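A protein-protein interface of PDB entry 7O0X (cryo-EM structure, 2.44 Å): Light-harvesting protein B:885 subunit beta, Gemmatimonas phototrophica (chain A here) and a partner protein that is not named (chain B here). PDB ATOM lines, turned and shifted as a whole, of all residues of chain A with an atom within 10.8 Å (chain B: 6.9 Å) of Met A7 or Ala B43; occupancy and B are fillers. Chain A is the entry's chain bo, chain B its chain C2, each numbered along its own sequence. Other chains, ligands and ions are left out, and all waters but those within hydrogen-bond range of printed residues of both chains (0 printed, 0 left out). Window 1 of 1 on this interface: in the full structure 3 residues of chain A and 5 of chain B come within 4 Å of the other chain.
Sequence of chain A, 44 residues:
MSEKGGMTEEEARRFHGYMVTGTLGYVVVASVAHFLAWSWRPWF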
ATOM      1  N   GLY A   6      29.345 -18.098   8.964  1.00  0.00           N
ATOM      2  CA  GLY A   6      28.592 -17.119   8.200  1.00  0.00           C
ATOM      3  C   GLY A   6      29.373 -15.852   7.909  1.00  0.00           C
ATOM      4  O   GLY A   6      30.399 -15.592   8.535  1.00  0.00           O
ATOM      5  N   MET A   7      28.885 -15.067   6.949  1.00  0.00           N
ATOM      6  CA  MET A   7      29.652 -13.946   6.421  1.00  0.00           C
ATOM      7  C   MET A   7      29.878 -12.864   7.471  1.00  0.00           C
ATOM      8  O   MET A   7      28.932 -12.391   8.108  1.00  0.00           O
ATOM      9  CB  MET A   7      28.960 -13.338   5.204  1.00  0.00           C
ATOM     10  CG  MET A   7      29.872 -12.375   4.461  1.00  0.00           C
ATOM     11  SD  MET A   7      29.115 -11.506   3.083  1.00  0.00           S
ATOM     12  CE  MET A   7      30.567 -11.154   2.098  1.00  0.00           C
ATOM     13  N   THR A   8      31.136 -12.478   7.644  1.00  0.00           N
ATOM     14  CA  THR A   8      31.532 -11.386   8.520  1.00  0.00           C
ATOM     15  C   THR A   8      31.751 -10.113   7.707  1.00  0.00           C
ATOM     16  O   THR A   8      31.800 -10.130   6.476  1.00  0.00           O
ATOM     17  CB  THR A   8      32.808 -11.748   9.285  1.00  0.00           C
ATOM     18  OG1 THR A   8      33.864 -12.003   8.351  1.00  0.00           O
ATOM     19  CG2 THR A   8      32.586 -12.989  10.133  1.00  0.00           C
ATOM     20  N   GLU A   9      31.879  -8.989   8.418  1.00  0.00           N
ATOM     21  CA  GLU A   9      32.273  -7.746   7.758  1.00  0.00           C
ATOM     22  C   GLU A   9      33.716  -7.804   7.268  1.00  0.00           C
ATOM     23  O   GLU A   9      34.068  -7.123   6.299  1.00  0.00           O
ATOM     24  CB  GLU A   9      32.070  -6.555   8.699  1.00  0.00           C
ATOM     25  CG  GLU A   9      32.371  -5.206   8.055  1.00  0.00           C
ATOM     26  CD  GLU A   9      31.799  -4.029   8.822  1.00  0.00           C
ATOM     27  OE1 GLU A   9      31.290  -4.232   9.944  1.00  0.00           O
ATOM     28  OE2 GLU A   9      31.859  -2.896   8.299  1.00  0.00           O
ATOM     29  N   GLU A  10      34.553  -8.617   7.914  1.00  0.00           N
ATOM     30  CA  GLU A  10      35.903  -8.860   7.415  1.00  0.00           C
ATOM     31  C   GLU A  10      35.877  -9.472   6.019  1.00  0.00           C
ATOM     32  O   GLU A  10      36.581  -9.014   5.114  1.00  0.00           O
ATOM     33  CB  GLU A  10      36.654  -9.773   8.386  1.00  0.00           C
ATOM     34  CG  GLU A  10      38.019 -10.233   7.899  1.00  0.00           C
ATOM     35  CD  GLU A  10      38.987  -9.087   7.691  1.00  0.00           C
ATOM     36  OE1 GLU A  10      38.964  -8.137   8.501  1.00  0.00           O
ATOM     37  OE2 GLU A  10      39.772  -9.137   6.722  1.00  0.00           O
ATOM     38  N   GLU A  11      35.073 -10.520   5.834  1.00  0.00           N
ATOM     39  CA  GLU A  11      34.931 -11.134   4.518  1.00  0.00           C
ATOM     40  C   GLU A  11      34.385 -10.153   3.486  1.00  0.00           C
ATOM     41  O   GLU A  11      34.807 -10.169   2.323  1.00  0.00           O
ATOM     42  CB  GLU A  11      34.033 -12.365   4.621  1.00  0.00           C
ATOM     43  CG  GLU A  11      34.723 -13.572   5.233  1.00  0.00           C
ATOM     44  CD  GLU A  11      33.750 -14.544   5.870  1.00  0.00           C
ATOM     45  OE1 GLU A  11      33.137 -14.184   6.897  1.00  0.00           O
ATOM     46  OE2 GLU A  11      33.602 -15.671   5.352  1.00  0.00           O
ATOM     47  N   ALA A  12      33.444  -9.294   3.884  1.00  0.00           N
ATOM     48  CA  ALA A  12      32.934  -8.278   2.968  1.00  0.00           C
ATOM     49  C   ALA A  12      34.021  -7.297   2.545  1.00  0.00           C
ATOM     50  O   ALA A  12      34.138  -6.963   1.360  1.00  0.00           O
ATOM     51  CB  ALA A  12      31.765  -7.534   3.613  1.00  0.00           C
ATOM     52  N   ARG A  13      34.826  -6.821   3.496  1.00  0.00           N
ATOM     53  CA  ARG A  13      35.905  -5.894   3.164  1.00  0.00           C
ATOM     54  C   ARG A  13      36.971  -6.559   2.301  1.00  0.00           C
ATOM     55  O   ARG A  13      37.512  -5.936   1.380  1.00  0.00           O
ATOM     56  CB  ARG A  13      36.526  -5.325   4.441  1.00  0.00           C
ATOM     57  CG  ARG A  13      37.270  -4.015   4.219  1.00  0.00           C
ATOM     58  CD  ARG A  13      38.337  -3.750   5.272  1.00  0.00           C
ATOM     59  NE  ARG A  13      39.451  -4.684   5.169  1.00  0.00           N
ATOM     60  CZ  ARG A  13      39.559  -5.807   5.864  1.00  0.00           C
ATOM     61  NH1 ARG A  13      38.850  -6.010   6.963  1.00  0.00           N
ATOM     62  NH2 ARG A  13      40.467  -6.708   5.502  1.00  0.00           N
ATOM     63  N   ARG A  14      37.285  -7.821   2.587  1.00  0.00           N
ATOM     64  CA  ARG A  14      38.212  -8.586   1.757  1.00  0.00           C
ATOM     65  C   ARG A  14      37.697  -8.750   0.329  1.00  0.00           C
ATOM     66  O   ARG A  14      38.431  -8.510  -0.636  1.00  0.00           O
ATOM     67  CB  ARG A  14      38.462  -9.946   2.404  1.00  0.00           C
ATOM     68  CG  ARG A  14      39.648 -10.708   1.858  1.00  0.00           C
ATOM     69  CD  ARG A  14      39.839 -11.997   2.635  1.00  0.00           C
ATOM     70  NE  ARG A  14      38.779 -12.955   2.344  1.00  0.00           N
ATOM     71  CZ  ARG A  14      38.274 -13.808   3.224  1.00  0.00           C
ATOM     72  NH1 ARG A  14      38.776 -13.923   4.442  1.00  0.00           N
ATOM     73  NH2 ARG A  14      37.252 -14.580   2.867  1.00  0.00           N
ATOM     74  N   PHE A  15      36.440  -9.169   0.173  1.00  0.00           N
ATOM     75  CA  PHE A  15      35.864  -9.310  -1.162  1.00  0.00           C
ATOM     76  C   PHE A  15      35.831  -7.983  -1.915  1.00  0.00           C
ATOM     77  O   PHE A  15      36.130  -7.934  -3.113  1.00  0.00           O
ATOM     78  CB  PHE A  15      34.457  -9.896  -1.069  1.00  0.00           C
ATOM     79  CG  PHE A  15      33.793 -10.072  -2.402  1.00  0.00           C
ATOM     80  CD1 PHE A  15      34.096 -11.158  -3.203  1.00  0.00           C
ATOM     81  CD2 PHE A  15      32.879  -9.140  -2.864  1.00  0.00           C
ATOM     82  CE1 PHE A  15      33.493 -11.318  -4.432  1.00  0.00           C
ATOM     83  CE2 PHE A  15      32.276  -9.293  -4.093  1.00  0.00           C
ATOM     84  CZ  PHE A  15      32.583 -10.384  -4.878  1.00  0.00           C
ATOM     85  N   HIS A  16      35.455  -6.902  -1.231  1.00  0.00           N
ATOM     86  CA  HIS A  16      35.394  -5.586  -1.861  1.00  0.00           C
ATOM     87  C   HIS A  16      36.737  -5.142  -2.432  1.00  0.00           C
ATOM     88  O   HIS A  16      36.784  -4.499  -3.487  1.00  0.00           O
ATOM     89  CB  HIS A  16      34.893  -4.558  -0.851  1.00  0.00           C
ATOM     90  CG  HIS A  16      34.609  -3.216  -1.445  1.00  0.00           C
ATOM     91  ND1 HIS A  16      33.540  -2.978  -2.281  1.00  0.00           N
ATOM     92  CD2 HIS A  16      35.262  -2.037  -1.324  1.00  0.00           C
ATOM     93  CE1 HIS A  16      33.546  -1.710  -2.647  1.00  0.00           C
ATOM     94  NE2 HIS A  16      34.581  -1.116  -2.080  1.00  0.00           N
ATOM     95  N   GLY A  17      37.838  -5.464  -1.752  1.00  0.00           N
ATOM     96  CA  GLY A  17      39.150  -5.138  -2.291  1.00  0.00           C
ATOM     97  C   GLY A  17      39.435  -5.792  -3.630  1.00  0.00           C
ATOM     98  O   GLY A  17      39.926  -5.147  -4.559  1.00  0.00           O
ATOM     99  N   MET A  19      37.084  -6.899  -5.711  1.00  0.00           N
ATOM    100  CA  MET A  19      36.128  -6.319  -6.651  1.00  0.00           C
ATOM    101  C   MET A  19      36.607  -4.981  -7.208  1.00  0.00           C
ATOM    102  O   MET A  19      36.509  -4.736  -8.415  1.00  0.00           O
ATOM    103  CB  MET A  19      34.770  -6.156  -5.970  1.00  0.00           C
ATOM    104  CG  MET A  19      33.710  -5.509  -6.842  1.00  0.00           C
ATOM    105  SD  MET A  19      33.183  -6.553  -8.210  1.00  0.00           S
ATOM    106  CE  MET A  19      32.136  -7.710  -7.337  1.00  0.00           C
ATOM    107  N   ARG B  40      20.846 -16.293   3.367  1.00  0.00           N
ATOM    108  CA  ARG B  40      22.203 -16.813   3.494  1.00  0.00           C
ATOM    109  C   ARG B  40      22.780 -16.574   4.892  1.00  0.00           C
ATOM    110  O   ARG B  40      22.446 -15.588   5.554  1.00  0.00           O
ATOM    111  CB  ARG B  40      23.107 -16.190   2.430  1.00  0.00           C
ATOM    112  CG  ARG B  40      23.240 -14.685   2.519  1.00  0.00           C
ATOM    113  CD  ARG B  40      24.105 -14.136   1.397  1.00  0.00           C
ATOM    114  NE  ARG B  40      24.087 -12.677   1.377  1.00  0.00           N
ATOM    115  CZ  ARG B  40      25.157 -11.906   1.503  1.00  0.00           C
ATOM    116  NH1 ARG B  40      26.370 -12.419   1.630  1.00  0.00           N
ATOM    117  NH2 ARG B  40      25.007 -10.585   1.496  1.00  0.00           N
ATOM    118  N   PRO B  41      23.644 -17.478   5.362  1.00  0.00           N
ATOM    119  CA  PRO B  41      24.221 -17.350   6.707  1.00  0.00           C
ATOM    120  C   PRO B  41      24.964 -16.035   6.887  1.00  0.00           C
ATOM    121  O   PRO B  41      25.837 -15.680   6.095  1.00  0.00           O
ATOM    122  CB  PRO B  41      25.168 -18.554   6.800  1.00  0.00           C
ATOM    123  CG  PRO B  41      24.587 -19.547   5.863  1.00  0.00           C
ATOM    124  CD  PRO B  41      24.082 -18.722   4.709  1.00  0.00           C
ATOM    125  N   MET B  42      24.612 -15.314   7.947  1.00  0.00           N
ATOM    126  CA  MET B  42      25.092 -13.959   8.174  1.00  0.00           C
ATOM    127  C   MET B  42      25.608 -13.843   9.600  1.00  0.00           C
ATOM    128  O   MET B  42      24.943 -14.288  10.540  1.00  0.00           O
ATOM    129  CB  MET B  42      23.975 -12.942   7.920  1.00  0.00           C
ATOM    130  CG  MET B  42      24.366 -11.496   8.147  1.00  0.00           C
ATOM    131  SD  MET B  42      25.783 -10.982   7.163  1.00  0.00           S
ATOM    132  CE  MET B  42      25.141 -11.195   5.504  1.00  0.00           C
ATOM    133  N   ALA B  43      26.794 -13.247   9.759  1.00  0.00           N
ATOM    134  CA  ALA B  43      27.401 -13.081  11.071  1.00  0.00           C
ATOM    135  C   ALA B  43      27.648 -11.631  11.455  1.00  0.00           C
ATOM    136  O   ALA B  43      27.782 -11.346  12.649  1.00  0.00           O
ATOM    137  CB  ALA B  43      28.732 -13.845  11.151  1.00  0.00           C
ATOM    138  N   ALA B  44      27.719 -10.716  10.494  1.00  0.00           N
ATOM    139  CA  ALA B  44      27.610  -9.299  10.793  1.00  0.00           C
ATOM    140  C   ALA B  44      26.147  -8.948  11.047  1.00  0.00           C
ATOM    141  O   ALA B  44      25.237  -9.690  10.671  1.00  0.00           O
ATOM    142  CB  ALA B  44      28.177  -8.459   9.651  1.00  0.00           C
ATOM    143  N   TRP B  45      25.918  -7.811  11.697  1.00  0.00           N
ATOM    144  CA  TRP B  45      24.550  -7.327  11.818  1.00  0.00           C
ATOM    145  C   TRP B  45      23.989  -6.941  10.455  1.00  0.00           C
ATOM    146  O   TRP B  45      24.681  -6.348   9.622  1.00  0.00           O
ATOM    147  CB  TRP B  45      24.466  -6.144  12.781  1.00  0.00           C
ATOM    148  CG  TRP B  45      23.086  -5.570  12.831  1.00  0.00           C
ATOM    149  CD1 TRP B  45      22.671  -4.393  12.280  1.00  0.00           C
ATOM    150  CD2 TRP B  45      21.917  -6.190  13.379  1.00  0.00           C
ATOM    151  NE1 TRP B  45      21.326  -4.219  12.495  1.00  0.00           N
ATOM    152  CE2 TRP B  45      20.838  -5.311  13.162  1.00  0.00           C
ATOM    153  CE3 TRP B  45      21.681  -7.395  14.048  1.00  0.00           C
ATOM    154  CZ2 TRP B  45      19.544  -5.598  13.591  1.00  0.00           C
ATOM    155  CZ3 TRP B  45      20.396  -7.677  14.472  1.00  0.00           C
ATOM    156  CH2 TRP B  45      19.344  -6.782  14.243  1.00  0.00           C
ATOM    157  N   SER B  46      22.720  -7.280  10.235  1.00  0.00           N
ATOM    158  CA  SER B  46      21.993  -6.845   9.045  1.00  0.00           C
ATOM    159  C   SER B  46      20.504  -6.889   9.348  1.00  0.00           C
ATOM    160  O   SER B  46      19.962  -7.964   9.621  1.00  0.00           O
ATOM    161  CB  SER B  46      22.327  -7.736   7.851  1.00  0.00           C
ATOM    162  OG  SER B  46      21.512  -7.420   6.737  1.00  0.00           O
ATOM    163  N   GLN B 103      21.263 -19.140  12.947  1.00  0.00           N
ATOM    164  CA  GLN B 103      21.249 -17.808  12.346  1.00  0.00           C
ATOM    165  C   GLN B 103      20.791 -16.744  13.337  1.00  0.00           C
ATOM    166  O   GLN B 103      21.361 -15.648  13.391  1.00  0.00           O
ATOM    167  CB  GLN B 103      20.349 -17.814  11.108  1.00  0.00           C
ATOM    168  CG  GLN B 103      20.210 -16.475  10.394  1.00  0.00           C
ATOM    169  CD  GLN B 103      21.367 -16.168   9.460  1.00  0.00           C
ATOM    170  OE1 GLN B 103      22.493 -16.611   9.677  1.00  0.00           O
ATOM    171  NE2 GLN B 103      21.087 -15.412   8.407  1.00  0.00           N
ATOM    172  N   ARG B 106      23.722 -15.928  15.765  1.00  0.00           N
ATOM    173  CA  ARG B 106      24.744 -15.100  15.126  1.00  0.00           C
ATOM    174  C   ARG B 106      24.326 -13.636  15.092  1.00  0.00           C
ATOM    175  O   ARG B 106      25.077 -12.747  15.510  1.00  0.00           O
ATOM    176  CB  ARG B 106      25.005 -15.576  13.697  1.00  0.00           C
ATOM    177  CG  ARG B 106      25.617 -16.944  13.538  1.00  0.00           C
ATOM    178  CD  ARG B 106      25.590 -17.328  12.066  1.00  0.00           C
ATOM    179  NE  ARG B 106      25.669 -18.767  11.860  1.00  0.00           N
ATOM    180  CZ  ARG B 106      24.835 -19.458  11.093  1.00  0.00           C
ATOM    181  NH1 ARG B 106      23.892 -18.863  10.384  1.00  0.00           N
ATOM    182  NH2 ARG B 106      24.969 -20.779  11.019  1.00  0.00           N
ATOM    183  N   LEU B 107      23.119 -13.374  14.590  1.00  0.00           N
ATOM    184  CA  LEU B 107      22.624 -12.008  14.465  1.00  0.00           C
ATOM    185  C   LEU B 107      22.440 -11.342  15.824  1.00  0.00           C
ATOM    186  O   LEU B 107      22.720 -10.148  15.978  1.00  0.00           O
ATOM    187  CB  LEU B 107      21.316 -12.012  13.678  1.00  0.00           C
ATOM    188  CG  LEU B 107      21.495 -12.441  12.220  1.00  0.00           C
ATOM    189  CD1 LEU B 107      20.159 -12.588  11.520  1.00  0.00           C
ATOM    190  CD2 LEU B 107      22.380 -11.452  11.481  1.00  0.00           C
ATOM    191  N   ALA B 109      24.166 -11.968  18.596  1.00  0.00           N
ATOM    192  CA  ALA B 109      25.506 -11.577  19.025  1.00  0.00           C
ATOM    193  C   ALA B 109      25.970 -10.307  18.318  1.00  0.00           C
ATOM    194  O   ALA B 109      26.498  -9.386  18.951  1.00  0.00           O
ATOM    195  CB  ALA B 109      26.488 -12.721  18.776  1.00  0.00           C
ATOM    196  N   ALA B 110      25.780 -10.243  16.998  1.00  0.00           N
ATOM    197  CA  ALA B 110      26.189  -9.068  16.232  1.00  0.00           C
ATOM    198  C   ALA B 110      25.380  -7.830  16.601  1.00  0.00           C
ATOM    199  O   ALA B 110      25.901  -6.711  16.539  1.00  0.00           O
ATOM    200  CB  ALA B 110      26.068  -9.355  14.736  1.00  0.00           C
ATOM    201  N   ARG B 111      24.112  -8.010  16.972  1.00  0.00           N
ATOM    202  CA  ARG B 111      23.276  -6.895  17.411  1.00  0.00           C
ATOM    203  C   ARG B 111      23.873  -6.179  18.615  1.00  0.00           C
ATOM    204  O   ARG B 111      23.937  -4.945  18.653  1.00  0.00           O
ATOM    205  CB  ARG B 111      21.873  -7.405  17.743  1.00  0.00           C
ATOM    206  CG  ARG B 111      20.835  -6.318  17.937  1.00  0.00           C
ATOM    207  CD  ARG B 111      19.516  -6.907  18.411  1.00  0.00           C
ATOM    208  NE  ARG B 111      19.619  -7.484  19.747  1.00  0.00           N
ATOM    209  CZ  ARG B 111      19.545  -6.793  20.877  1.00  0.00           C
ATOM    210  NH1 ARG B 111      19.425  -5.476  20.876  1.00  0.00           N
ATOM    211  NH2 ARG B 111      19.608  -7.439  22.037  1.00  0.00           N
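Hydrophobic or aromatic side chains of chain B that line the printed part of chain A: Pro B41, Met B42, Ala B43 and Ala B44.
Among the printed residues, 8 pairs touch across the chains.
Among the printed residues, no Asp or Glu carboxylate lies within 4 Å of a Lys or Arg side-chain nitrogen of the other chain.
O of Arg B40 lies within hydrogen-bond range of NE2 of Gln B103 (3.2 Å).
The backbone NH (N) of Met B42 lies within hydrogen-bond range of the side-chain amide oxygen (OE1) of Gln B103, 3.0 Å away.
Met A7 touches just these residues of chain B: Arg B40, Pro B41, Met B42, Ala B43 and Ala B44.
Of the printed residues of chain A, Ala B43 touches Gly A6 (3.6 Å) and Met A7 (2.8 Å).
Of chain A, only Gly A6 and Met A7 come within 4 Å of Pro B41.
Printed residues of chain A within 4 Å of Met B42: Met A7 (3.6 Å).
Printed residues of chain A within 4 Å of Ala B44: Met A7 (3.2 Å) and Glu A9 (3.9 Å).
Of the printed residues of chain B, Glu A9 touches Ala B44.
Of the printed residues of chain A, Arg B40 touches Met A7 (3.2 Å).
Of the printed residues of chain B, Gly A6 touches Pro B41 (3.8 Å) and Ala B43 (3.6 Å).
The nearest residue of chain A that does not touch Ala B43 is Thr A8 (4.1 Å).
The side-chain sulfur (SD) of Met A7 is in hydrogen-bond range of the guanidinium group (NH1) of Arg B40.
The backbone carbonyl oxygen (O) of Pro B41 sits at hydrogen-bond distance from the backbone NH (N) of Met A7.
The backbone carbonyl oxygen (O) of Met A7 lies within hydrogen-bond range of the backbone NH (N) of Ala B43 (2.8 Å).
The backbone carbonyl oxygen (O) of Met A7 is in hydrogen-bond range of the backbone NH (N) of Ala B44.
The backbone carbonyl oxygen (O) of Met A7 sits close to the side-chain sulfur (SD) of Met B42, at 3.6 Å.
Among the printed residues, merely in contact across the chains: Gly A6 with Pro B41 (3.8 Å), Gly A6 with Ala B43 (3.6 Å) and Glu A9 with Ala B44 (3.9 Å).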
